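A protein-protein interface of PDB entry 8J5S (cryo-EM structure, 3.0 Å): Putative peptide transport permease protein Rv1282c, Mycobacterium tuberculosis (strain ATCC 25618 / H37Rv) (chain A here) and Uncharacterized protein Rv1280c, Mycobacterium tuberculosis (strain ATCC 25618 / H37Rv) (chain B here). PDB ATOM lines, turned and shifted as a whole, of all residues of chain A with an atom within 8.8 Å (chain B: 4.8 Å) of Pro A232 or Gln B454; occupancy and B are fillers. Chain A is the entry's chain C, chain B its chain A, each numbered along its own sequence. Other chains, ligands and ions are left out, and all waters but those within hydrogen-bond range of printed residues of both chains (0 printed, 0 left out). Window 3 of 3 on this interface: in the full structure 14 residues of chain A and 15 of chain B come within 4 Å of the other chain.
NE2 of His B455 is in hydrogen-bond range of O of Asp A47, at 3.2 Å.
The side-chain hydroxyl (OG1) of Thr B456 lies within hydrogen-bond range of the backbone carbonyl oxygen (O) of Ile B452, at 3.3 Å. The backbone carbonyl oxygen (O) of Leu B464 sits close to the side-chain amide oxygen (OE1) of Gln B454 (3.4 Å). OH of Tyr A46 is in hydrogen-bond range of O of Pro A232, at 3.2 Å. The side-chain amide nitrogen (NE2) of Gln A76 sits close to the backbone NH (N) of Asp A47 (3.5 Å).
CD1 of Ile B452 touches CD1 of Leu A49, 3.9 Å away. CD1 of Leu A49 touches ND1 of His B455, at 3.6 Å. Leu A69 touches Gln B451 (CD2 to CB, 3.6 Å). Leu A69 touches Ile B452. Pro A231 touches Gln B454. Pro A232 touches Gln B454 (N to NE2, 3.9997 Å).
Printed residues of chain A within 4 Å of Gln B454: Pro A231 and Pro A232. Of the printed residues of chain B, Asp A47 touches His B455 (3.2 Å). Of the printed residues of chain B, Leu A69 touches Gln B451 (3.6 Å) and Ile B452 (3.6 Å). Of the printed residues of chain A, Ile B452 touches Leu A49 (3.9 Å) and Leu A69 (3.6 Å). Printed residues of chain A within 4 Å of Gln B451: Leu A69. Tyr A46 touches none of the printed residues of chain B.
Hydrophobic or aromatic side chains of chain B that line the printed part of chain A: Ile B452 and His B455.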
ATOM      1  N   TYR A  46      19.274 -17.763   5.533  1.00  0.00           N
ATOM      2  CA  TYR A  46      19.443 -16.449   4.950  1.00  0.00           C
ATOM      3  C   TYR A  46      20.852 -15.961   5.264  1.00  0.00           C
ATOM      4  O   TYR A  46      21.600 -16.608   5.997  1.00  0.00           O
ATOM      5  CB  TYR A  46      18.345 -15.527   5.482  1.00  0.00           C
ATOM      6  CG  TYR A  46      18.640 -14.054   5.528  1.00  0.00           C
ATOM      7  CD1 TYR A  46      18.536 -13.271   4.392  1.00  0.00           C
ATOM      8  CD2 TYR A  46      18.989 -13.436   6.721  1.00  0.00           C
ATOM      9  CE1 TYR A  46      18.796 -11.918   4.432  1.00  0.00           C
ATOM     10  CE2 TYR A  46      19.254 -12.085   6.772  1.00  0.00           C
ATOM     11  CZ  TYR A  46      19.155 -11.330   5.625  1.00  0.00           C
ATOM     12  OH  TYR A  46      19.415  -9.984   5.673  1.00  0.00           O
ATOM     13  N   ASP A  47      21.242 -14.855   4.636  1.00  0.00           N
ATOM     14  CA  ASP A  47      22.455 -14.086   4.916  1.00  0.00           C
ATOM     15  C   ASP A  47      23.748 -14.880   4.747  1.00  0.00           C
ATOM     16  O   ASP A  47      24.812 -14.392   5.138  1.00  0.00           O
ATOM     17  CB  ASP A  47      22.425 -13.439   6.318  1.00  0.00           C
ATOM     18  CG  ASP A  47      22.625 -14.437   7.469  1.00  0.00           C
ATOM     19  OD1 ASP A  47      23.430 -15.377   7.344  1.00  0.00           O
ATOM     20  OD2 ASP A  47      21.962 -14.294   8.518  1.00  0.00           O
ATOM     21  N   ASP A  48      23.709 -16.093   4.201  1.00  0.00           N
ATOM     22  CA  ASP A  48      24.933 -16.844   3.964  1.00  0.00           C
ATOM     23  C   ASP A  48      25.048 -17.174   2.486  1.00  0.00           C
ATOM     24  O   ASP A  48      24.049 -17.474   1.829  1.00  0.00           O
ATOM     25  CB  ASP A  48      25.005 -18.108   4.831  1.00  0.00           C
ATOM     26  CG  ASP A  48      24.070 -19.192   4.381  1.00  0.00           C
ATOM     27  OD1 ASP A  48      24.386 -19.887   3.395  1.00  0.00           O
ATOM     28  OD2 ASP A  48      23.027 -19.374   5.035  1.00  0.00           O
ATOM     29  N   LEU A  49      26.274 -17.103   1.969  1.00  0.00           N
ATOM     30  CA  LEU A  49      26.548 -17.150   0.542  1.00  0.00           C
ATOM     31  C   LEU A  49      27.149 -18.490   0.149  1.00  0.00           C
ATOM     32  O   LEU A  49      28.006 -19.027   0.854  1.00  0.00           O
ATOM     33  CB  LEU A  49      27.511 -16.037   0.138  1.00  0.00           C
ATOM     34  CG  LEU A  49      27.218 -14.623   0.623  1.00  0.00           C
ATOM     35  CD1 LEU A  49      28.218 -13.628   0.079  1.00  0.00           C
ATOM     36  CD2 LEU A  49      25.879 -14.244   0.181  1.00  0.00           C
ATOM     37  N   LEU A  69      25.049 -13.129  -6.289  1.00  0.00           N
ATOM     38  CA  LEU A  69      25.998 -13.221  -5.189  1.00  0.00           C
ATOM     39  C   LEU A  69      25.963 -14.565  -4.481  1.00  0.00           C
ATOM     40  O   LEU A  69      26.644 -14.733  -3.471  1.00  0.00           O
ATOM     41  CB  LEU A  69      25.734 -12.109  -4.181  1.00  0.00           C
ATOM     42  CG  LEU A  69      26.041 -10.688  -4.629  1.00  0.00           C
ATOM     43  CD1 LEU A  69      24.812 -10.024  -5.209  1.00  0.00           C
ATOM     44  CD2 LEU A  69      26.552  -9.907  -3.460  1.00  0.00           C
ATOM     45  N   GLN A  71      23.233 -16.162  -3.088  1.00  0.00           N
ATOM     46  CA  GLN A  71      22.255 -16.284  -2.021  1.00  0.00           C
ATOM     47  C   GLN A  71      21.068 -17.105  -2.485  1.00  0.00           C
ATOM     48  O   GLN A  71      20.617 -16.969  -3.621  1.00  0.00           O
ATOM     49  CB  GLN A  71      21.776 -14.907  -1.573  1.00  0.00           C
ATOM     50  CG  GLN A  71      22.837 -14.109  -0.903  1.00  0.00           C
ATOM     51  CD  GLN A  71      22.650 -12.624  -0.999  1.00  0.00           C
ATOM     52  OE1 GLN A  71      21.933 -12.141  -1.861  1.00  0.00           O
ATOM     53  NE2 GLN A  71      23.303 -11.891  -0.130  1.00  0.00           N
ATOM     54  N   GLN A  76      16.005 -15.505   1.098  1.00  0.00           N
ATOM     55  CA  GLN A  76      16.026 -14.056   0.951  1.00  0.00           C
ATOM     56  C   GLN A  76      14.622 -13.501   0.809  1.00  0.00           C
ATOM     57  O   GLN A  76      14.276 -12.496   1.436  1.00  0.00           O
ATOM     58  CB  GLN A  76      16.869 -13.646  -0.254  1.00  0.00           C
ATOM     59  CG  GLN A  76      18.283 -14.132  -0.235  1.00  0.00           C
ATOM     60  CD  GLN A  76      19.149 -13.353   0.700  1.00  0.00           C
ATOM     61  OE1 GLN A  76      19.169 -12.129   0.663  1.00  0.00           O
ATOM     62  NE2 GLN A  76      19.888 -14.057   1.548  1.00  0.00           N
ATOM     63  N   ARG A  79      12.680 -13.625   4.149  1.00  0.00           N
ATOM     64  CA  ARG A  79      13.051 -12.535   5.049  1.00  0.00           C
ATOM     65  C   ARG A  79      12.499 -11.199   4.561  1.00  0.00           C
ATOM     66  O   ARG A  79      11.969 -10.401   5.351  1.00  0.00           O
ATOM     67  CB  ARG A  79      14.570 -12.487   5.186  1.00  0.00           C
ATOM     68  CG  ARG A  79      15.125 -11.325   5.975  1.00  0.00           C
ATOM     69  CD  ARG A  79      14.323 -11.006   7.208  1.00  0.00           C
ATOM     70  NE  ARG A  79      15.146 -10.431   8.259  1.00  0.00           N
ATOM     71  CZ  ARG A  79      15.772 -11.153   9.175  1.00  0.00           C
ATOM     72  NH1 ARG A  79      16.506 -10.562  10.099  1.00  0.00           N
ATOM     73  NH2 ARG A  79      15.653 -12.469   9.165  1.00  0.00           N
ATOM     74  N   LYS A  83       9.788  -8.591   6.614  1.00  0.00           N
ATOM     75  CA  LYS A  83       9.895  -7.160   6.882  1.00  0.00           C
ATOM     76  C   LYS A  83       8.790  -6.378   6.185  1.00  0.00           C
ATOM     77  O   LYS A  83       8.127  -5.532   6.798  1.00  0.00           O
ATOM     78  CB  LYS A  83      11.268  -6.647   6.461  1.00  0.00           C
ATOM     79  CG  LYS A  83      12.312  -6.818   7.533  1.00  0.00           C
ATOM     80  CD  LYS A  83      13.337  -5.712   7.487  1.00  0.00           C
ATOM     81  CE  LYS A  83      14.509  -6.041   8.378  1.00  0.00           C
ATOM     82  NZ  LYS A  83      15.572  -6.723   7.608  1.00  0.00           N
ATOM     83  N   LYS A 141      17.477   6.458   8.307  1.00  0.00           N
ATOM     84  CA  LYS A 141      17.870   5.633   7.172  1.00  0.00           C
ATOM     85  C   LYS A 141      18.841   4.537   7.570  1.00  0.00           C
ATOM     86  O   LYS A 141      18.720   3.405   7.097  1.00  0.00           O
ATOM     87  CB  LYS A 141      18.502   6.490   6.078  1.00  0.00           C
ATOM     88  CG  LYS A 141      18.410   5.885   4.702  1.00  0.00           C
ATOM     89  CD  LYS A 141      18.649   6.921   3.630  1.00  0.00           C
ATOM     90  CE  LYS A 141      20.111   6.998   3.253  1.00  0.00           C
ATOM     91  NZ  LYS A 141      20.481   5.956   2.266  1.00  0.00           N
ATOM     92  N   ASN A 142      19.804   4.852   8.432  1.00  0.00           N
ATOM     93  CA  ASN A 142      20.819   3.899   8.850  1.00  0.00           C
ATOM     94  C   ASN A 142      20.641   3.481  10.303  1.00  0.00           C
ATOM     95  O   ASN A 142      21.616   3.195  10.999  1.00  0.00           O
ATOM     96  CB  ASN A 142      22.212   4.472   8.615  1.00  0.00           C
ATOM     97  CG  ASN A 142      22.612   4.434   7.156  1.00  0.00           C
ATOM     98  OD1 ASN A 142      22.308   5.346   6.393  1.00  0.00           O
ATOM     99  ND2 ASN A 142      23.294   3.369   6.759  1.00  0.00           N
ATOM    100  N   SER A 143      19.399   3.450  10.773  1.00  0.00           N
ATOM    101  CA  SER A 143      19.078   2.943  12.094  1.00  0.00           C
ATOM    102  C   SER A 143      18.745   1.459  12.014  1.00  0.00           C
ATOM    103  O   SER A 143      18.436   0.924  10.949  1.00  0.00           O
ATOM    104  CB  SER A 143      17.909   3.712  12.700  1.00  0.00           C
ATOM    105  OG  SER A 143      16.685   3.313  12.115  1.00  0.00           O
ATOM    106  N   ALA A 144      18.814   0.793  13.167  1.00  0.00           N
ATOM    107  CA  ALA A 144      18.553  -0.641  13.219  1.00  0.00           C
ATOM    108  C   ALA A 144      17.060  -0.934  13.270  1.00  0.00           C
ATOM    109  O   ALA A 144      16.516  -1.603  12.387  1.00  0.00           O
ATOM    110  CB  ALA A 144      19.260  -1.260  14.424  1.00  0.00           C
ATOM    111  N   ILE A 229      14.971   0.783   3.450  1.00  0.00           N
ATOM    112  CA  ILE A 229      15.643  -0.376   4.028  1.00  0.00           C
ATOM    113  C   ILE A 229      16.980  -0.587   3.336  1.00  0.00           C
ATOM    114  O   ILE A 229      17.077  -0.507   2.108  1.00  0.00           O
ATOM    115  CB  ILE A 229      14.745  -1.623   3.942  1.00  0.00           C
ATOM    116  CG1 ILE A 229      13.753  -1.617   5.100  1.00  0.00           C
ATOM    117  CG2 ILE A 229      15.562  -2.876   3.982  1.00  0.00           C
ATOM    118  CD1 ILE A 229      12.739  -2.709   5.048  1.00  0.00           C
ATOM    119  N   GLN A 230      18.018  -0.858   4.135  1.00  0.00           N
ATOM    120  CA  GLN A 230      19.423  -0.744   3.757  1.00  0.00           C
ATOM    121  C   GLN A 230      20.022  -2.064   3.270  1.00  0.00           C
ATOM    122  O   GLN A 230      19.329  -3.080   3.295  1.00  0.00           O
ATOM    123  CB  GLN A 230      20.183  -0.161   4.948  1.00  0.00           C
ATOM    124  CG  GLN A 230      19.971   1.333   5.090  1.00  0.00           C
ATOM    125  CD  GLN A 230      19.869   2.052   3.753  1.00  0.00           C
ATOM    126  OE1 GLN A 230      20.711   1.883   2.874  1.00  0.00           O
ATOM    127  NE2 GLN A 230      18.828   2.848   3.591  1.00  0.00           N
ATOM    128  N   PRO A 231      21.266  -2.097   2.789  1.00  0.00           N
ATOM    129  CA  PRO A 231      21.757  -3.278   2.058  1.00  0.00           C
ATOM    130  C   PRO A 231      21.898  -4.535   2.903  1.00  0.00           C
ATOM    131  O   PRO A 231      21.519  -5.613   2.422  1.00  0.00           O
ATOM    132  CB  PRO A 231      23.121  -2.819   1.528  1.00  0.00           C
ATOM    133  CG  PRO A 231      22.976  -1.376   1.383  1.00  0.00           C
ATOM    134  CD  PRO A 231      22.169  -0.953   2.565  1.00  0.00           C
ATOM    135  N   PRO A 232      22.478  -4.490   4.111  1.00  0.00           N
ATOM    136  CA  PRO A 232      22.758  -5.768   4.791  1.00  0.00           C
ATOM    137  C   PRO A 232      21.525  -6.622   4.993  1.00  0.00           C
ATOM    138  O   PRO A 232      21.619  -7.853   4.948  1.00  0.00           O
ATOM    139  CB  PRO A 232      23.366  -5.334   6.128  1.00  0.00           C
ATOM    140  CG  PRO A 232      22.859  -3.971   6.334  1.00  0.00           C
ATOM    141  CD  PRO A 232      22.829  -3.358   4.979  1.00  0.00           C
ATOM    142  N   ASP A 233      20.368  -6.005   5.190  1.00  0.00           N
ATOM    143  CA  ASP A 233      19.107  -6.695   5.383  1.00  0.00           C
ATOM    144  C   ASP A 233      18.194  -6.443   4.192  1.00  0.00           C
ATOM    145  O   ASP A 233      18.349  -5.467   3.465  1.00  0.00           O
ATOM    146  CB  ASP A 233      18.444  -6.238   6.675  1.00  0.00           C
ATOM    147  CG  ASP A 233      17.882  -4.856   6.571  1.00  0.00           C
ATOM    148  OD1 ASP A 233      16.667  -4.732   6.334  1.00  0.00           O
ATOM    149  OD2 ASP A 233      18.650  -3.888   6.729  1.00  0.00           O
ATOM    150  N   VAL A 234      17.237  -7.338   3.987  1.00  0.00           N
ATOM    151  CA  VAL A 234      16.480  -7.362   2.745  1.00  0.00           C
ATOM    152  C   VAL A 234      15.039  -6.950   2.985  1.00  0.00           C
ATOM    153  O   VAL A 234      14.492  -7.101   4.078  1.00  0.00           O
ATOM    154  CB  VAL A 234      16.534  -8.746   2.077  1.00  0.00           C
ATOM    155  CG1 VAL A 234      17.879  -8.962   1.432  1.00  0.00           C
ATOM    156  CG2 VAL A 234      16.284  -9.805   3.088  1.00  0.00           C
ATOM    157  N   SER A 235      14.434  -6.407   1.937  1.00  0.00           N
ATOM    158  CA  SER A 235      13.008  -6.157   1.854  1.00  0.00           C
ATOM    159  C   SER A 235      12.556  -6.594   0.476  1.00  0.00           C
ATOM    160  O   SER A 235      13.371  -6.929  -0.382  1.00  0.00           O
ATOM    161  CB  SER A 235      12.668  -4.691   2.088  1.00  0.00           C
ATOM    162  OG  SER A 235      11.344  -4.410   1.693  1.00  0.00           O
ATOM    163  N   THR A 238      13.761  -4.018  -2.192  1.00  0.00           N
ATOM    164  CA  THR A 238      15.184  -4.129  -2.486  1.00  0.00           C
ATOM    165  C   THR A 238      15.468  -5.348  -3.345  1.00  0.00           C
ATOM    166  O   THR A 238      16.309  -5.296  -4.245  1.00  0.00           O
ATOM    167  CB  THR A 238      15.997  -4.187  -1.196  1.00  0.00           C
ATOM    168  OG1 THR A 238      15.979  -5.516  -0.680  1.00  0.00           O
ATOM    169  CG2 THR A 238      15.427  -3.251  -0.166  1.00  0.00           C
ATOM    170  N   ALA B 450      31.221  -4.386  -3.002  1.00  0.00           N
ATOM    171  CA  ALA B 450      30.869  -3.832  -1.705  1.00  0.00           C
ATOM    172  C   ALA B 450      30.084  -4.828  -0.872  1.00  0.00           C
ATOM    173  O   ALA B 450      30.339  -4.978   0.326  1.00  0.00           O
ATOM    174  CB  ALA B 450      30.068  -2.551  -1.895  1.00  0.00           C
ATOM    175  N   GLN B 451      29.125  -5.520  -1.483  1.00  0.00           N
ATOM    176  CA  GLN B 451      28.320  -6.470  -0.724  1.00  0.00           C
ATOM    177  C   GLN B 451      29.153  -7.645  -0.240  1.00  0.00           C
ATOM    178  O   GLN B 451      29.026  -8.059   0.916  1.00  0.00           O
ATOM    179  CB  GLN B 451      27.144  -6.949  -1.560  1.00  0.00           C
ATOM    180  CG  GLN B 451      26.408  -5.830  -2.240  1.00  0.00           C
ATOM    181  CD  GLN B 451      24.934  -6.078  -2.368  1.00  0.00           C
ATOM    182  OE1 GLN B 451      24.269  -6.426  -1.398  1.00  0.00           O
ATOM    183  NE2 GLN B 451      24.406  -5.901  -3.571  1.00  0.00           N
ATOM    184  N   ILE B 452      30.017  -8.195  -1.092  1.00  0.00           N
ATOM    185  CA  ILE B 452      30.866  -9.296  -0.642  1.00  0.00           C
ATOM    186  C   ILE B 452      31.797  -8.828   0.463  1.00  0.00           C
ATOM    187  O   ILE B 452      32.010  -9.535   1.454  1.00  0.00           O
ATOM    188  CB  ILE B 452      31.656  -9.906  -1.811  1.00  0.00           C
ATOM    189  CG1 ILE B 452      30.732 -10.277  -2.960  1.00  0.00           C
ATOM    190  CG2 ILE B 452      32.393 -11.136  -1.352  1.00  0.00           C
ATOM    191  CD1 ILE B 452      29.771 -11.373  -2.633  1.00  0.00           C
ATOM    192  N   ALA B 453      32.373  -7.636   0.314  1.00  0.00           N
ATOM    193  CA  ALA B 453      33.303  -7.134   1.315  1.00  0.00           C
ATOM    194  C   ALA B 453      32.616  -6.908   2.648  1.00  0.00           C
ATOM    195  O   ALA B 453      33.166  -7.246   3.698  1.00  0.00           O
ATOM    196  CB  ALA B 453      33.954  -5.845   0.828  1.00  0.00           C
ATOM    197  N   GLN B 454      31.409  -6.346   2.637  1.00  0.00           N
ATOM    198  CA  GLN B 454      30.723  -6.105   3.898  1.00  0.00           C
ATOM    199  C   GLN B 454      30.262  -7.406   4.534  1.00  0.00           C
ATOM    200  O   GLN B 454      30.321  -7.552   5.759  1.00  0.00           O
ATOM    201  CB  GLN B 454      29.555  -5.144   3.701  1.00  0.00           C
ATOM    202  CG  GLN B 454      28.284  -5.754   3.219  1.00  0.00           C
ATOM    203  CD  GLN B 454      27.104  -4.840   3.418  1.00  0.00           C
ATOM    204  OE1 GLN B 454      27.076  -4.043   4.346  1.00  0.00           O
ATOM    205  NE2 GLN B 454      26.125  -4.938   2.531  1.00  0.00           N
ATOM    206  N   HIS B 455      29.830  -8.377   3.730  1.00  0.00           N
ATOM    207  CA  HIS B 455      29.467  -9.666   4.300  1.00  0.00           C
ATOM    208  C   HIS B 455      30.667 -10.330   4.947  1.00  0.00           C
ATOM    209  O   HIS B 455      30.562 -10.862   6.052  1.00  0.00           O
ATOM    210  CB  HIS B 455      28.863 -10.573   3.235  1.00  0.00           C
ATOM    211  CG  HIS B 455      28.629 -11.974   3.704  1.00  0.00           C
ATOM    212  ND1 HIS B 455      29.451 -13.023   3.355  1.00  0.00           N
ATOM    213  CD2 HIS B 455      27.667 -12.499   4.495  1.00  0.00           C
ATOM    214  CE1 HIS B 455      29.007 -14.133   3.913  1.00  0.00           C
ATOM    215  NE2 HIS B 455      27.925 -13.842   4.611  1.00  0.00           N
ATOM    216  N   THR B 456      31.823 -10.293   4.291  1.00  0.00           N
ATOM    217  CA  THR B 456      32.999 -10.933   4.866  1.00  0.00           C
ATOM    218  C   THR B 456      33.511 -10.176   6.081  1.00  0.00           C
ATOM    219  O   THR B 456      34.026 -10.791   7.019  1.00  0.00           O
ATOM    220  CB  THR B 456      34.091 -11.066   3.808  1.00  0.00           C
ATOM    221  OG1 THR B 456      33.681 -12.016   2.821  1.00  0.00           O
ATOM    222  CG2 THR B 456      35.372 -11.554   4.420  1.00  0.00           C
ATOM    223  N   LEU B 457      33.371  -8.853   6.098  1.00  0.00           N
ATOM    224  CA  LEU B 457      33.851  -8.073   7.232  1.00  0.00           C
ATOM    225  C   LEU B 457      32.945  -8.206   8.443  1.00  0.00           C
ATOM    226  O   LEU B 457      33.425  -8.119   9.573  1.00  0.00           O
ATOM    227  CB  LEU B 457      33.989  -6.606   6.839  1.00  0.00           C
ATOM    228  CG  LEU B 457      35.337  -6.211   6.247  1.00  0.00           C
ATOM    229  CD1 LEU B 457      35.288  -4.796   5.750  1.00  0.00           C
ATOM    230  CD2 LEU B 457      36.425  -6.373   7.272  1.00  0.00           C
ATOM    231  N   ALA B 458      31.647  -8.425   8.234  1.00  0.00           N
ATOM    232  CA  ALA B 458      30.748  -8.650   9.359  1.00  0.00           C
ATOM    233  C   ALA B 458      31.158  -9.860  10.185  1.00  0.00           C
ATOM    234  O   ALA B 458      30.840  -9.930  11.373  1.00  0.00           O
ATOM    235  CB  ALA B 458      29.320  -8.817   8.856  1.00  0.00           C
ATOM    236  N   LYS B 463      31.645  -3.018  10.785  1.00  0.00           N
ATOM    237  CA  LYS B 463      30.539  -2.507   9.992  1.00  0.00           C
ATOM    238  C   LYS B 463      31.074  -1.686   8.831  1.00  0.00           C
ATOM    239  O   LYS B 463      31.886  -0.780   9.024  1.00  0.00           O
ATOM    240  CB  LYS B 463      29.599  -1.659  10.840  1.00  0.00           C
ATOM    241  CG  LYS B 463      28.383  -1.192  10.084  1.00  0.00           C
ATOM    242  CD  LYS B 463      27.208  -0.967  11.000  1.00  0.00           C
ATOM    243  CE  LYS B 463      25.939  -0.764  10.199  1.00  0.00           C
ATOM    244  NZ  LYS B 463      25.948  -1.557   8.934  1.00  0.00           N
ATOM    245  N   LEU B 464      30.628  -2.013   7.629  1.00  0.00           N
ATOM    246  CA  LEU B 464      31.021  -1.307   6.416  1.00  0.00           C
ATOM    247  C   LEU B 464      29.772  -0.641   5.866  1.00  0.00           C
ATOM    248  O   LEU B 464      28.912  -1.302   5.289  1.00  0.00           O
ATOM    249  CB  LEU B 464      31.645  -2.259   5.401  1.00  0.00           C
ATOM    250  CG  LEU B 464      32.128  -1.628   4.099  1.00  0.00           C
ATOM    251  CD1 LEU B 464      33.503  -1.040   4.269  1.00  0.00           C
ATOM    252  CD2 LEU B 464      32.126  -2.637   2.985  1.00  0.00           C
ATOM    253  N   LEU B 466      27.773   1.334   3.270  1.00  0.00           N
ATOM    254  CA  LEU B 466      27.879   1.529   1.833  1.00  0.00           C
ATOM    255  C   LEU B 466      27.234   2.847   1.438  1.00  0.00           C
ATOM    256  O   LEU B 466      26.121   3.153   1.867  1.00  0.00           O
ATOM    257  CB  LEU B 466      27.215   0.377   1.083  1.00  0.00           C
ATOM    258  CG  LEU B 466      27.739  -1.029   1.345  1.00  0.00           C
ATOM    259  CD1 LEU B 466      27.197  -1.972   0.304  1.00  0.00           C
ATOM    260  CD2 LEU B 466      29.244  -1.045   1.337  1.00  0.00           C
